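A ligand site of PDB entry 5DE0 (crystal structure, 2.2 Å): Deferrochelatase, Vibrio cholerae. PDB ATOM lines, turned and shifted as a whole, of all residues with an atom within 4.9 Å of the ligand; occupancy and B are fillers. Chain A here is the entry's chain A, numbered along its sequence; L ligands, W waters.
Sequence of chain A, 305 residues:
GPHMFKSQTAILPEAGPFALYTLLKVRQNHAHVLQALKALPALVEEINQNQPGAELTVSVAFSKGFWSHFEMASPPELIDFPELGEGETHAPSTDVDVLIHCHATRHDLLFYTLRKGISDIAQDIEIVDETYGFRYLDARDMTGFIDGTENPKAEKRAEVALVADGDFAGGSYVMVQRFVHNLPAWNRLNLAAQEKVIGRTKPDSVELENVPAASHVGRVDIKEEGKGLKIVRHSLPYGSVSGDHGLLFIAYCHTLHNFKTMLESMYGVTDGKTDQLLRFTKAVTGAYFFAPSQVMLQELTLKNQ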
ATOM      1  N   ASP A 141     -25.386  -6.822  12.207  1.00  0.00           N
ATOM      2  CA  ASP A 141     -25.904  -5.476  12.086  1.00  0.00           C
ATOM      3  C   ASP A 141     -26.762  -5.412  10.827  1.00  0.00           C
ATOM      4  O   ASP A 141     -26.640  -6.259   9.945  1.00  0.00           O
ATOM      5  CB  ASP A 141     -24.769  -4.450  12.040  1.00  0.00           C
ATOM      6  CG  ASP A 141     -25.260  -3.022  11.883  1.00  0.00           C
ATOM      7  OD1 ASP A 141     -25.490  -2.353  12.909  1.00  0.00           O
ATOM      8  OD2 ASP A 141     -25.423  -2.582  10.728  1.00  0.00           O
ATOM      9  N   THR A 143     -26.541  -3.716   8.362  1.00  0.00           N
ATOM     10  CA  THR A 143     -25.736  -3.538   7.156  1.00  0.00           C
ATOM     11  C   THR A 143     -25.402  -4.890   6.521  1.00  0.00           C
ATOM     12  O   THR A 143     -24.921  -4.958   5.394  1.00  0.00           O
ATOM     13  CB  THR A 143     -24.419  -2.795   7.461  1.00  0.00           C
ATOM     14  OG1 THR A 143     -23.732  -3.439   8.544  1.00  0.00           O
ATOM     15  CG2 THR A 143     -24.696  -1.339   7.833  1.00  0.00           C
ATOM     16  N   PHE A 145     -23.380  -7.067   8.069  1.00  0.00           N
ATOM     17  CA  PHE A 145     -22.114  -7.495   8.653  1.00  0.00           C
ATOM     18  C   PHE A 145     -22.287  -7.875  10.119  1.00  0.00           C
ATOM     19  O   PHE A 145     -23.031  -7.218  10.854  1.00  0.00           O
ATOM     20  CB  PHE A 145     -21.063  -6.383   8.516  1.00  0.00           C
ATOM     21  CG  PHE A 145     -20.495  -6.244   7.131  1.00  0.00           C
ATOM     22  CD1 PHE A 145     -21.245  -5.650   6.123  1.00  0.00           C
ATOM     23  CD2 PHE A 145     -19.220  -6.677   6.845  1.00  0.00           C
ATOM     24  CE1 PHE A 145     -20.725  -5.519   4.851  1.00  0.00           C
ATOM     25  CE2 PHE A 145     -18.691  -6.545   5.567  1.00  0.00           C
ATOM     26  CZ  PHE A 145     -19.439  -5.966   4.576  1.00  0.00           C
ATOM     27  N   ILE A 146     -21.611  -8.930  10.534  1.00  0.00           N
ATOM     28  CA  ILE A 146     -21.679  -9.405  11.909  1.00  0.00           C
ATOM     29  C   ILE A 146     -21.070  -8.391  12.877  1.00  0.00           C
ATOM     30  O   ILE A 146     -19.992  -7.841  12.618  1.00  0.00           O
ATOM     31  CB  ILE A 146     -20.960 -10.761  12.067  1.00  0.00           C
ATOM     32  CG1 ILE A 146     -21.582 -11.813  11.140  1.00  0.00           C
ATOM     33  CG2 ILE A 146     -21.006 -11.236  13.515  1.00  0.00           C
ATOM     34  CD1 ILE A 146     -20.935 -13.174  11.211  1.00  0.00           C
ATOM     35  N   ASP A 147     -21.765  -8.136  13.977  1.00  0.00           N
ATOM     36  CA  ASP A 147     -21.288  -7.215  14.994  1.00  0.00           C
ATOM     37  C   ASP A 147     -20.967  -7.935  16.300  1.00  0.00           C
ATOM     38  O   ASP A 147     -21.835  -8.579  16.894  1.00  0.00           O
ATOM     39  CB  ASP A 147     -22.325  -6.119  15.250  1.00  0.00           C
ATOM     40  CG  ASP A 147     -21.894  -5.139  16.329  1.00  0.00           C
ATOM     41  OD1 ASP A 147     -20.766  -4.618  16.251  1.00  0.00           O
ATOM     42  OD2 ASP A 147     -22.695  -4.897  17.252  1.00  0.00           O
ATOM     43  N   GLY A 148     -19.719  -7.814  16.750  1.00  0.00           N
ATOM     44  CA  GLY A 148     -19.300  -8.396  18.022  1.00  0.00           C
ATOM     45  C   GLY A 148     -18.292  -9.512  17.901  1.00  0.00           C
ATOM     46  O   GLY A 148     -18.014 -10.214  18.874  1.00  0.00           O
ATOM     47  N   THR A 149     -17.720  -9.676  16.712  1.00  0.00           N
ATOM     48  CA  THR A 149     -16.760 -10.751  16.445  1.00  0.00           C
ATOM     49  C   THR A 149     -15.522 -10.649  17.336  1.00  0.00           C
ATOM     50  O   THR A 149     -15.085 -11.645  17.927  1.00  0.00           O
ATOM     51  CB  THR A 149     -16.311 -10.756  14.974  1.00  0.00           C
ATOM     52  OG1 THR A 149     -17.448 -10.971  14.126  1.00  0.00           O
ATOM     53  CG2 THR A 149     -15.293 -11.861  14.725  1.00  0.00           C
ATOM     54  N   GLU A 150     -14.963  -9.448  17.453  1.00  0.00           N
ATOM     55  CA  GLU A 150     -13.768  -9.233  18.245  1.00  0.00           C
ATOM     56  C   GLU A 150     -14.083  -8.623  19.601  1.00  0.00           C
ATOM     57  O   GLU A 150     -13.199  -8.116  20.295  1.00  0.00           O
ATOM     58  CB  GLU A 150     -12.777  -8.339  17.490  1.00  0.00           C
ATOM     59  CG  GLU A 150     -12.277  -8.947  16.184  1.00  0.00           C
ATOM     60  CD  GLU A 150     -11.465 -10.211  16.388  1.00  0.00           C
ATOM     61  OE1 GLU A 150     -10.852 -10.351  17.467  1.00  0.00           O
ATOM     62  OE2 GLU A 150     -11.443 -11.067  15.479  1.00  0.00           O
ATOM     63  N   ASN A 151     -15.354  -8.661  19.982  1.00  0.00           N
ATOM     64  CA  ASN A 151     -15.781  -8.201  21.292  1.00  0.00           C
ATOM     65  C   ASN A 151     -15.220  -9.120  22.373  1.00  0.00           C
ATOM     66  O   ASN A 151     -15.292 -10.346  22.241  1.00  0.00           O
ATOM     67  CB  ASN A 151     -17.311  -8.135  21.377  1.00  0.00           C
ATOM     68  CG  ASN A 151     -17.805  -7.121  22.400  1.00  0.00           C
ATOM     69  OD1 ASN A 151     -17.251  -6.034  22.528  1.00  0.00           O
ATOM     70  ND2 ASN A 151     -18.854  -7.488  23.129  1.00  0.00           N
ATOM     71  N   MET A 175     -20.383   4.929  27.073  1.00  0.00           N
ATOM     72  CA  MET A 175     -20.660   5.798  25.934  1.00  0.00           C
ATOM     73  C   MET A 175     -21.868   5.262  25.161  1.00  0.00           C
ATOM     74  O   MET A 175     -22.040   4.055  25.036  1.00  0.00           O
ATOM     75  CB  MET A 175     -19.447   5.929  25.009  1.00  0.00           C
ATOM     76  CG  MET A 175     -19.094   4.660  24.252  1.00  0.00           C
ATOM     77  SD  MET A 175     -18.042   4.996  22.816  1.00  0.00           S
ATOM     78  CE  MET A 175     -19.124   6.019  21.829  1.00  0.00           C
ATOM     79  N   GLN A 177     -24.331   5.972  21.558  1.00  0.00           N
ATOM     80  CA  GLN A 177     -24.627   6.651  20.308  1.00  0.00           C
ATOM     81  C   GLN A 177     -25.697   5.909  19.514  1.00  0.00           C
ATOM     82  O   GLN A 177     -25.486   4.752  19.135  1.00  0.00           O
ATOM     83  CB  GLN A 177     -23.370   6.813  19.455  1.00  0.00           C
ATOM     84  CG  GLN A 177     -22.454   7.955  19.868  1.00  0.00           C
ATOM     85  CD  GLN A 177     -21.258   8.085  18.938  1.00  0.00           C
ATOM     86  OE1 GLN A 177     -20.459   7.163  18.796  1.00  0.00           O
ATOM     87  NE2 GLN A 177     -21.135   9.243  18.289  1.00  0.00           N
ATOM     88  N   PHE A 179     -27.335   5.291  16.137  1.00  0.00           N
ATOM     89  CA  PHE A 179     -27.027   5.513  14.733  1.00  0.00           C
ATOM     90  C   PHE A 179     -28.240   5.278  13.838  1.00  0.00           C
ATOM     91  O   PHE A 179     -29.055   4.384  14.099  1.00  0.00           O
ATOM     92  CB  PHE A 179     -25.879   4.610  14.292  1.00  0.00           C
ATOM     93  CG  PHE A 179     -24.546   4.999  14.851  1.00  0.00           C
ATOM     94  CD1 PHE A 179     -24.126   4.524  16.090  1.00  0.00           C
ATOM     95  CD2 PHE A 179     -23.693   5.837  14.140  1.00  0.00           C
ATOM     96  CE1 PHE A 179     -22.893   4.891  16.604  1.00  0.00           C
ATOM     97  CE2 PHE A 179     -22.464   6.196  14.648  1.00  0.00           C
ATOM     98  CZ  PHE A 179     -22.061   5.720  15.882  1.00  0.00           C
ATOM     99  N   HIS A 181     -29.143   4.353   9.953  1.00  0.00           N
ATOM    100  CA  HIS A 181     -28.530   3.824   8.732  1.00  0.00           C
ATOM    101  C   HIS A 181     -29.204   4.311   7.455  1.00  0.00           C
ATOM    102  O   HIS A 181     -30.429   4.473   7.402  1.00  0.00           O
ATOM    103  CB  HIS A 181     -28.574   2.292   8.748  1.00  0.00           C
ATOM    104  CG  HIS A 181     -27.653   1.665   9.737  1.00  0.00           C
ATOM    105  ND1 HIS A 181     -26.984   2.400  10.707  1.00  0.00           N
ATOM    106  CD2 HIS A 181     -27.299   0.372   9.936  1.00  0.00           C
ATOM    107  CE1 HIS A 181     -26.253   1.577  11.440  1.00  0.00           C
ATOM    108  NE2 HIS A 181     -26.422   0.350  11.003  1.00  0.00           N
ATOM    109  N   ILE A 198     -16.048  -1.661   5.816  1.00  0.00           N
ATOM    110  CA  ILE A 198     -16.082  -2.224   7.158  1.00  0.00           C
ATOM    111  C   ILE A 198     -14.684  -2.628   7.604  1.00  0.00           C
ATOM    112  O   ILE A 198     -14.202  -2.175   8.641  1.00  0.00           O
ATOM    113  CB  ILE A 198     -17.010  -3.451   7.236  1.00  0.00           C
ATOM    114  CG1 ILE A 198     -18.466  -3.035   6.957  1.00  0.00           C
ATOM    115  CG2 ILE A 198     -16.908  -4.115   8.601  1.00  0.00           C
ATOM    116  CD1 ILE A 198     -19.015  -2.054   7.972  1.00  0.00           C
ATOM    117  N   ARG A 200     -13.791  -6.112   7.125  1.00  0.00           N
ATOM    118  CA  ARG A 200     -13.871  -7.572   7.250  1.00  0.00           C
ATOM    119  C   ARG A 200     -14.719  -8.143   6.118  1.00  0.00           C
ATOM    120  O   ARG A 200     -15.416  -7.403   5.415  1.00  0.00           O
ATOM    121  CB  ARG A 200     -14.462  -7.975   8.603  1.00  0.00           C
ATOM    122  CG  ARG A 200     -13.732  -7.390   9.814  1.00  0.00           C
ATOM    123  CD  ARG A 200     -14.320  -7.898  11.125  1.00  0.00           C
ATOM    124  NE  ARG A 200     -13.893  -9.258  11.432  1.00  0.00           N
ATOM    125  CZ  ARG A 200     -12.878  -9.558  12.234  1.00  0.00           C
ATOM    126  NH1 ARG A 200     -12.184  -8.590  12.812  1.00  0.00           N
ATOM    127  NH2 ARG A 200     -12.563 -10.820  12.454  1.00  0.00           N
ATOM    128  N   SER A 205     -17.210 -12.661   8.523  1.00  0.00           N
ATOM    129  CA  SER A 205     -16.533 -11.658   9.351  1.00  0.00           C
ATOM    130  C   SER A 205     -15.041 -11.912   9.556  1.00  0.00           C
ATOM    131  O   SER A 205     -14.503 -11.690  10.642  1.00  0.00           O
ATOM    132  CB  SER A 205     -17.221 -11.559  10.721  1.00  0.00           C
ATOM    133  OG  SER A 205     -16.743 -10.445  11.451  1.00  0.00           O
ATOM    134  N   HIS A 216     -13.784   1.216   8.988  1.00  0.00           N
ATOM    135  CA  HIS A 216     -14.262   1.314  10.359  1.00  0.00           C
ATOM    136  C   HIS A 216     -13.363   0.572  11.336  1.00  0.00           C
ATOM    137  O   HIS A 216     -13.025   1.096  12.397  1.00  0.00           O
ATOM    138  CB  HIS A 216     -15.689   0.777  10.483  1.00  0.00           C
ATOM    139  CG  HIS A 216     -16.287   1.028  11.825  1.00  0.00           C
ATOM    140  ND1 HIS A 216     -16.567   2.290  12.292  1.00  0.00           N
ATOM    141  CD2 HIS A 216     -16.622   0.175  12.826  1.00  0.00           C
ATOM    142  CE1 HIS A 216     -17.067   2.211  13.517  1.00  0.00           C
ATOM    143  NE2 HIS A 216     -17.107   0.934  13.856  1.00  0.00           N
ATOM    144  N   VAL A 217     -12.977  -0.647  10.972  1.00  0.00           N
ATOM    145  CA  VAL A 217     -12.043  -1.418  11.783  1.00  0.00           C
ATOM    146  C   VAL A 217     -10.727  -0.656  11.886  1.00  0.00           C
ATOM    147  O   VAL A 217     -10.141  -0.549  12.967  1.00  0.00           O
ATOM    148  CB  VAL A 217     -11.788  -2.814  11.188  1.00  0.00           C
ATOM    149  CG1 VAL A 217     -10.635  -3.497  11.915  1.00  0.00           C
ATOM    150  CG2 VAL A 217     -13.048  -3.660  11.282  1.00  0.00           C
ATOM    151  N   VAL A 220     -11.081   2.135  14.535  1.00  0.00           N
ATOM    152  CA  VAL A 220     -11.311   1.780  15.937  1.00  0.00           C
ATOM    153  C   VAL A 220     -10.300   0.768  16.478  1.00  0.00           C
ATOM    154  O   VAL A 220     -10.183   0.592  17.693  1.00  0.00           O
ATOM    155  CB  VAL A 220     -12.730   1.228  16.147  1.00  0.00           C
ATOM    156  CG1 VAL A 220     -13.763   2.270  15.741  1.00  0.00           C
ATOM    157  CG2 VAL A 220     -12.926  -0.065  15.386  1.00  0.00           C
ATOM    158  N   ASP A 221      -9.578   0.091  15.587  1.00  0.00           N
ATOM    159  CA  ASP A 221      -8.490  -0.796  16.003  1.00  0.00           C
ATOM    160  C   ASP A 221      -7.256   0.060  16.288  1.00  0.00           C
ATOM    161  O   ASP A 221      -6.358   0.166  15.450  1.00  0.00           O
ATOM    162  CB  ASP A 221      -8.197  -1.850  14.936  1.00  0.00           C
ATOM    163  CG  ASP A 221      -7.269  -2.933  15.430  1.00  0.00           C
ATOM    164  OD1 ASP A 221      -7.128  -3.092  16.661  1.00  0.00           O
ATOM    165  OD2 ASP A 221      -6.688  -3.652  14.584  1.00  0.00           O
ATOM    166  N   LYS A 230      -9.149  -1.697  24.146  1.00  0.00           N
ATOM    167  CA  LYS A 230     -10.336  -2.540  24.077  1.00  0.00           C
ATOM    168  C   LYS A 230     -11.517  -1.961  24.857  1.00  0.00           C
ATOM    169  O   LYS A 230     -11.344  -1.296  25.880  1.00  0.00           O
ATOM    170  CB  LYS A 230     -10.008  -3.936  24.606  1.00  0.00           C
ATOM    171  CG  LYS A 230      -9.058  -4.726  23.708  1.00  0.00           C
ATOM    172  CD  LYS A 230      -9.693  -4.993  22.356  1.00  0.00           C
ATOM    173  CE  LYS A 230      -8.714  -5.658  21.400  1.00  0.00           C
ATOM    174  NZ  LYS A 230      -7.597  -4.746  21.017  1.00  0.00           N
ATOM    175  N   ILE A 231     -12.713  -2.211  24.342  1.00  0.00           N
ATOM    176  CA  ILE A 231     -13.954  -1.827  25.007  1.00  0.00           C
ATOM    177  C   ILE A 231     -14.926  -2.999  25.009  1.00  0.00           C
ATOM    178  O   ILE A 231     -14.785  -3.925  24.217  1.00  0.00           O
ATOM    179  CB  ILE A 231     -14.625  -0.609  24.322  1.00  0.00           C
ATOM    180  CG1 ILE A 231     -15.048  -0.961  22.900  1.00  0.00           C
ATOM    181  CG2 ILE A 231     -13.701   0.595  24.330  1.00  0.00           C
ATOM    182  CD1 ILE A 231     -15.755   0.170  22.176  1.00  0.00           C
ATOM    183  N   ARG A 233     -18.560  -3.898  24.156  1.00  0.00           N
ATOM    184  CA  ARG A 233     -19.732  -3.394  23.444  1.00  0.00           C
ATOM    185  C   ARG A 233     -20.993  -4.183  23.765  1.00  0.00           C
ATOM    186  O   ARG A 233     -20.993  -5.418  23.702  1.00  0.00           O
ATOM    187  CB  ARG A 233     -19.470  -3.409  21.935  1.00  0.00           C
ATOM    188  CG  ARG A 233     -18.522  -2.320  21.453  1.00  0.00           C
ATOM    189  CD  ARG A 233     -18.133  -2.544  20.006  1.00  0.00           C
ATOM    190  NE  ARG A 233     -17.258  -3.708  19.859  1.00  0.00           N
ATOM    191  CZ  ARG A 233     -17.194  -4.456  18.764  1.00  0.00           C
ATOM    192  NH1 ARG A 233     -17.955  -4.168  17.716  1.00  0.00           N
ATOM    193  NH2 ARG A 233     -16.373  -5.499  18.711  1.00  0.00           N
ATOM    194  N   LEU A 247     -28.159   0.886  14.454  1.00  0.00           N
ATOM    195  CA  LEU A 247     -27.508   0.287  15.609  1.00  0.00           C
ATOM    196  C   LEU A 247     -27.477   1.240  16.799  1.00  0.00           C
ATOM    197  O   LEU A 247     -27.042   2.385  16.682  1.00  0.00           O
ATOM    198  CB  LEU A 247     -26.071  -0.136  15.253  1.00  0.00           C
ATOM    199  CG  LEU A 247     -25.230  -0.774  16.364  1.00  0.00           C
ATOM    200  CD1 LEU A 247     -25.705  -2.190  16.647  1.00  0.00           C
ATOM    201  CD2 LEU A 247     -23.753  -0.767  15.989  1.00  0.00           C
ATOM    202  N   PHE A 249     -25.425   1.935  19.491  1.00  0.00           N
ATOM    203  CA  PHE A 249     -24.095   1.657  20.015  1.00  0.00           C
ATOM    204  C   PHE A 249     -23.983   2.057  21.479  1.00  0.00           C
ATOM    205  O   PHE A 249     -24.266   3.193  21.845  1.00  0.00           O
ATOM    206  CB  PHE A 249     -23.018   2.377  19.197  1.00  0.00           C
ATOM    207  CG  PHE A 249     -21.619   2.030  19.622  1.00  0.00           C
ATOM    208  CD1 PHE A 249     -20.978   0.925  19.077  1.00  0.00           C
ATOM    209  CD2 PHE A 249     -20.964   2.793  20.564  1.00  0.00           C
ATOM    210  CE1 PHE A 249     -19.699   0.596  19.471  1.00  0.00           C
ATOM    211  CE2 PHE A 249     -19.676   2.464  20.968  1.00  0.00           C
ATOM    212  CZ  PHE A 249     -19.047   1.365  20.425  1.00  0.00           C
ATOM    213  N   PHE A 259     -12.801   5.462  24.614  1.00  0.00           N
ATOM    214  CA  PHE A 259     -13.941   5.990  23.866  1.00  0.00           C
ATOM    215  C   PHE A 259     -13.551   7.248  23.083  1.00  0.00           C
ATOM    216  O   PHE A 259     -13.790   7.341  21.881  1.00  0.00           O
ATOM    217  CB  PHE A 259     -15.109   6.332  24.802  1.00  0.00           C
ATOM    218  CG  PHE A 259     -15.661   5.138  25.542  1.00  0.00           C
ATOM    219  CD1 PHE A 259     -15.548   3.862  25.029  1.00  0.00           C
ATOM    220  CD2 PHE A 259     -16.319   5.315  26.754  1.00  0.00           C
ATOM    221  CE1 PHE A 259     -16.070   2.779  25.711  1.00  0.00           C
ATOM    222  CE2 PHE A 259     -16.836   4.226  27.441  1.00  0.00           C
ATOM    223  CZ  PHE A 259     -16.713   2.958  26.910  1.00  0.00           C
ATOM    224  N   MET A 262     -11.169   6.547  20.118  1.00  0.00           N
ATOM    225  CA  MET A 262     -11.851   5.914  18.989  1.00  0.00           C
ATOM    226  C   MET A 262     -12.720   6.903  18.223  1.00  0.00           C
ATOM    227  O   MET A 262     -12.751   6.895  16.991  1.00  0.00           O
ATOM    228  CB  MET A 262     -12.708   4.734  19.474  1.00  0.00           C
ATOM    229  CG  MET A 262     -11.905   3.560  19.994  1.00  0.00           C
ATOM    230  SD  MET A 262     -12.953   2.278  20.706  1.00  0.00           S
ATOM    231  CE  MET A 262     -11.708   1.110  21.255  1.00  0.00           C
ATOM    232  N   LEU A 263     -13.429   7.755  18.965  1.00  0.00           N
ATOM    233  CA  LEU A 263     -14.307   8.745  18.361  1.00  0.00           C
ATOM    234  C   LEU A 263     -13.521   9.833  17.636  1.00  0.00           C
ATOM    235  O   LEU A 263     -13.973  10.335  16.597  1.00  0.00           O
ATOM    236  CB  LEU A 263     -15.211   9.364  19.432  1.00  0.00           C
ATOM    237  CG  LEU A 263     -16.361   8.483  19.905  1.00  0.00           C
ATOM    238  CD1 LEU A 263     -17.049   9.090  21.110  1.00  0.00           C
ATOM    239  CD2 LEU A 263     -17.356   8.275  18.773  1.00  0.00           C
ATOM    240  N   MET A 266     -12.469   8.181  14.415  1.00  0.00           N
ATOM    241  CA  MET A 266     -13.576   7.978  13.495  1.00  0.00           C
ATOM    242  C   MET A 266     -14.016   9.248  12.782  1.00  0.00           C
ATOM    243  O   MET A 266     -14.302   9.237  11.587  1.00  0.00           O
ATOM    244  CB  MET A 266     -14.774   7.370  14.231  1.00  0.00           C
ATOM    245  CG  MET A 266     -14.640   5.897  14.548  1.00  0.00           C
ATOM    246  SD  MET A 266     -16.089   5.276  15.419  1.00  0.00           S
ATOM    247  CE  MET A 266     -17.389   5.749  14.283  1.00  0.00           C
ATOM    248  N   LEU A 277     -17.494   4.257   7.163  1.00  0.00           N
ATOM    249  CA  LEU A 277     -18.805   3.725   7.539  1.00  0.00           C
ATOM    250  C   LEU A 277     -19.798   4.846   7.804  1.00  0.00           C
ATOM    251  O   LEU A 277     -21.008   4.672   7.628  1.00  0.00           O
ATOM    252  CB  LEU A 277     -18.669   2.819   8.769  1.00  0.00           C
ATOM    253  CG  LEU A 277     -19.948   2.200   9.343  1.00  0.00           C
ATOM    254  CD1 LEU A 277     -20.638   1.329   8.298  1.00  0.00           C
ATOM    255  CD2 LEU A 277     -19.621   1.404  10.583  1.00  0.00           C
ATOM    256  N   THR A 281     -24.147   5.846   7.596  1.00  0.00           N
ATOM    257  CA  THR A 281     -24.894   5.956   8.848  1.00  0.00           C
ATOM    258  C   THR A 281     -24.546   7.250   9.557  1.00  0.00           C
ATOM    259  O   THR A 281     -23.441   7.785   9.406  1.00  0.00           O
ATOM    260  CB  THR A 281     -24.629   4.757   9.785  1.00  0.00           C
ATOM    261  OG1 THR A 281     -25.453   4.870  10.946  1.00  0.00           O
ATOM    262  CG2 THR A 281     -23.163   4.729  10.210  1.00  0.00           C
HETATM  263  C1  LIG L   1     -15.768  -3.548  15.172  1.00  0.00           C
HETATM  264  C2  LIG L   1     -19.880  -2.093  13.019  1.00  0.00           C
HETATM  265  C3  LIG L   1     -19.777   2.015  15.616  1.00  0.00           C
HETATM  266  C4  LIG L   1     -15.983   0.357  18.143  1.00  0.00           C
HETATM  267  C5  LIG L   1     -16.876  -3.497  14.349  1.00  0.00           C
HETATM  268  C6  LIG L   1     -17.245  -4.495  13.358  1.00  0.00           C
HETATM  269  C7  LIG L   1     -18.381  -4.090  12.769  1.00  0.00           C
HETATM  270  C8  LIG L   1     -18.767  -2.827  13.360  1.00  0.00           C
HETATM  271  C9  LIG L   1     -19.142  -4.831  11.656  1.00  0.00           C
HETATM  272  C10 LIG L   1     -16.465  -5.784  13.048  1.00  0.00           C
HETATM  273  C11 LIG L   1     -17.031  -6.939  13.871  1.00  0.00           C
HETATM  274  C12 LIG L   1     -16.512  -6.854  15.292  1.00  0.00           C
HETATM  275  O1  LIG L   1     -15.297  -7.099  15.494  1.00  0.00           O
HETATM  276  O2  LIG L   1     -17.316  -6.549  16.205  1.00  0.00           O
HETATM  277  C13 LIG L   1     -20.213  -0.851  13.531  1.00  0.00           C
HETATM  278  C14 LIG L   1     -21.364  -0.056  13.136  1.00  0.00           C
HETATM  279  C15 LIG L   1     -21.337   1.080  13.861  1.00  0.00           C
HETATM  280  C16 LIG L   1     -20.169   1.034  14.725  1.00  0.00           C
HETATM  281  C17 LIG L   1     -22.380  -0.509  12.071  1.00  0.00           C
HETATM  282  C18 LIG L   1     -22.311   2.295  13.848  1.00  0.00           C
HETATM  283  C19 LIG L   1     -23.342   2.432  13.003  1.00  0.00           C
HETATM  284  C20 LIG L   1     -18.721   1.943  16.500  1.00  0.00           C
HETATM  285  C21 LIG L   1     -18.269   3.009  17.365  1.00  0.00           C
HETATM  286  C22 LIG L   1     -17.214   2.558  18.069  1.00  0.00           C
HETATM  287  C23 LIG L   1     -16.968   1.178  17.654  1.00  0.00           C
HETATM  288  C24 LIG L   1     -18.938   4.400  17.430  1.00  0.00           C
HETATM  289  C25 LIG L   1     -16.345   3.267  19.150  1.00  0.00           C
HETATM  290  C26 LIG L   1     -16.550   4.508  19.611  1.00  0.00           C
HETATM  291  C27 LIG L   1     -15.577  -0.856  17.615  1.00  0.00           C
HETATM  292  C28 LIG L   1     -14.519  -1.678  18.144  1.00  0.00           C
HETATM  293  C29 LIG L   1     -14.447  -2.898  17.213  1.00  0.00           C
HETATM  294  C30 LIG L   1     -15.467  -2.693  16.218  1.00  0.00           C
HETATM  295  C31 LIG L   1     -13.642  -1.406  19.378  1.00  0.00           C
HETATM  296  C32 LIG L   1     -13.470  -4.095  17.342  1.00  0.00           C
HETATM  297  C33 LIG L   1     -12.325  -3.911  16.341  1.00  0.00           C
HETATM  298  C34 LIG L   1     -11.256  -4.946  16.588  1.00  0.00           C
HETATM  299  O3  LIG L   1     -11.086  -5.846  15.725  1.00  0.00           O
HETATM  300  O4  LIG L   1     -10.579  -4.873  17.649  1.00  0.00           O
HETATM  301  N1  LIG L   1     -17.826  -2.499  14.319  1.00  0.00           N
HETATM  302  N2  LIG L   1     -19.508  -0.155  14.491  1.00  0.00           N
HETATM  303  N3  LIG L   1     -17.904   0.843  16.701  1.00  0.00           N
HETATM  304  N4  LIG L   1     -16.108  -1.482  16.480  1.00  0.00           N
HETATM  305 FE1  LIG L   1     -17.829  -0.853  15.518  1.00  0.00          FE
HETATM  306  O   HOH W   1     -18.222  -7.912  10.528  1.00  0.00           O
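An oxygen (O2) of the ligand lies within salt-bridge range of the guanidinium group (NH2) of Arg 233 (2.9 Å).
The backbone NH (N) of Thr 149 is in hydrogen-bond range of an oxygen (O2) of the ligand, at 3.2 Å.
A ring nitrogen (NE2) of His 216 binds an iron atom (FE1) of the ligand, at 2.5 Å.
N of Gly 148 sits at hydrogen-bond distance from O2 of the ligand, at 2.8 Å.
O1 of the ligand sits at hydrogen-bond distance from N of Glu 150, 3.1 Å away.
N of His 216 is in hydrogen-bond range of O of Ile 198, at 3.4 Å.
NH2 of Arg 200 lies within salt-bridge range of OE2 of Glu 150 (3.2 Å).
N of Val 217 lies within hydrogen-bond range of O of Ile 198 (3.0 Å).
N of Gln 177 lies within hydrogen-bond range of O of Phe 249 (2.8 Å).
The backbone carbonyl oxygen (O) of Ser 205 is in hydrogen-bond range of the guanidinium group (NE) of Arg 200, at 2.6 Å.
A ring nitrogen (ND1) of His 181 lies within hydrogen-bond range of the side-chain hydroxyl of Thr 281 (2.9 Å).
The backbone NH (N) of Phe 179 lies within hydrogen-bond range of the backbone carbonyl oxygen (O) of Leu 247 (3.0 Å).
The backbone NH (N) of Arg 233 lies within hydrogen-bond range of the side-chain amide oxygen (OD1) of Asn 151 (3.0 Å).
Merely in contact with the ligand: Phe 249 (3.2 Å), Ile 146 (3.3 Å), Phe 179 (3.4 Å), His 181 (3.4 Å), Leu 277 (3.4 Å), Gln 177 (3.4 Å), Val 220 (3.6 Å), Met 175 (3.6 Å), Arg 200 (3.6 Å), Met 266 (3.6 Å), Thr 281 (3.6 Å), Met 262 (3.7 Å), Asp 141 (3.7 Å), Leu 247 (3.7 Å), Ile 231 (3.8 Å), Ile 198 (3.9 Å), Asp 147 (3.9 Å), Leu 263 (3.9 Å) and Phe 145 (3.99 Å).
Hydrophobic or aromatic side chains that line the ligand: Phe 145, Met 175, Phe 179, His 181, Ile 198, His 216, Val 220, Ile 231, Leu 247, Phe 249, Met 262, Leu 263, Met 266 and Leu 277.
Of the 31 residues printed, 24 come within 4 Å of the ligand.
Water W1 bridges the backbone carbonyl oxygen (O) of Ile 146 (2.7 Å) and the side-chain hydroxyl (OG) of Ser 205 (3.1 Å).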
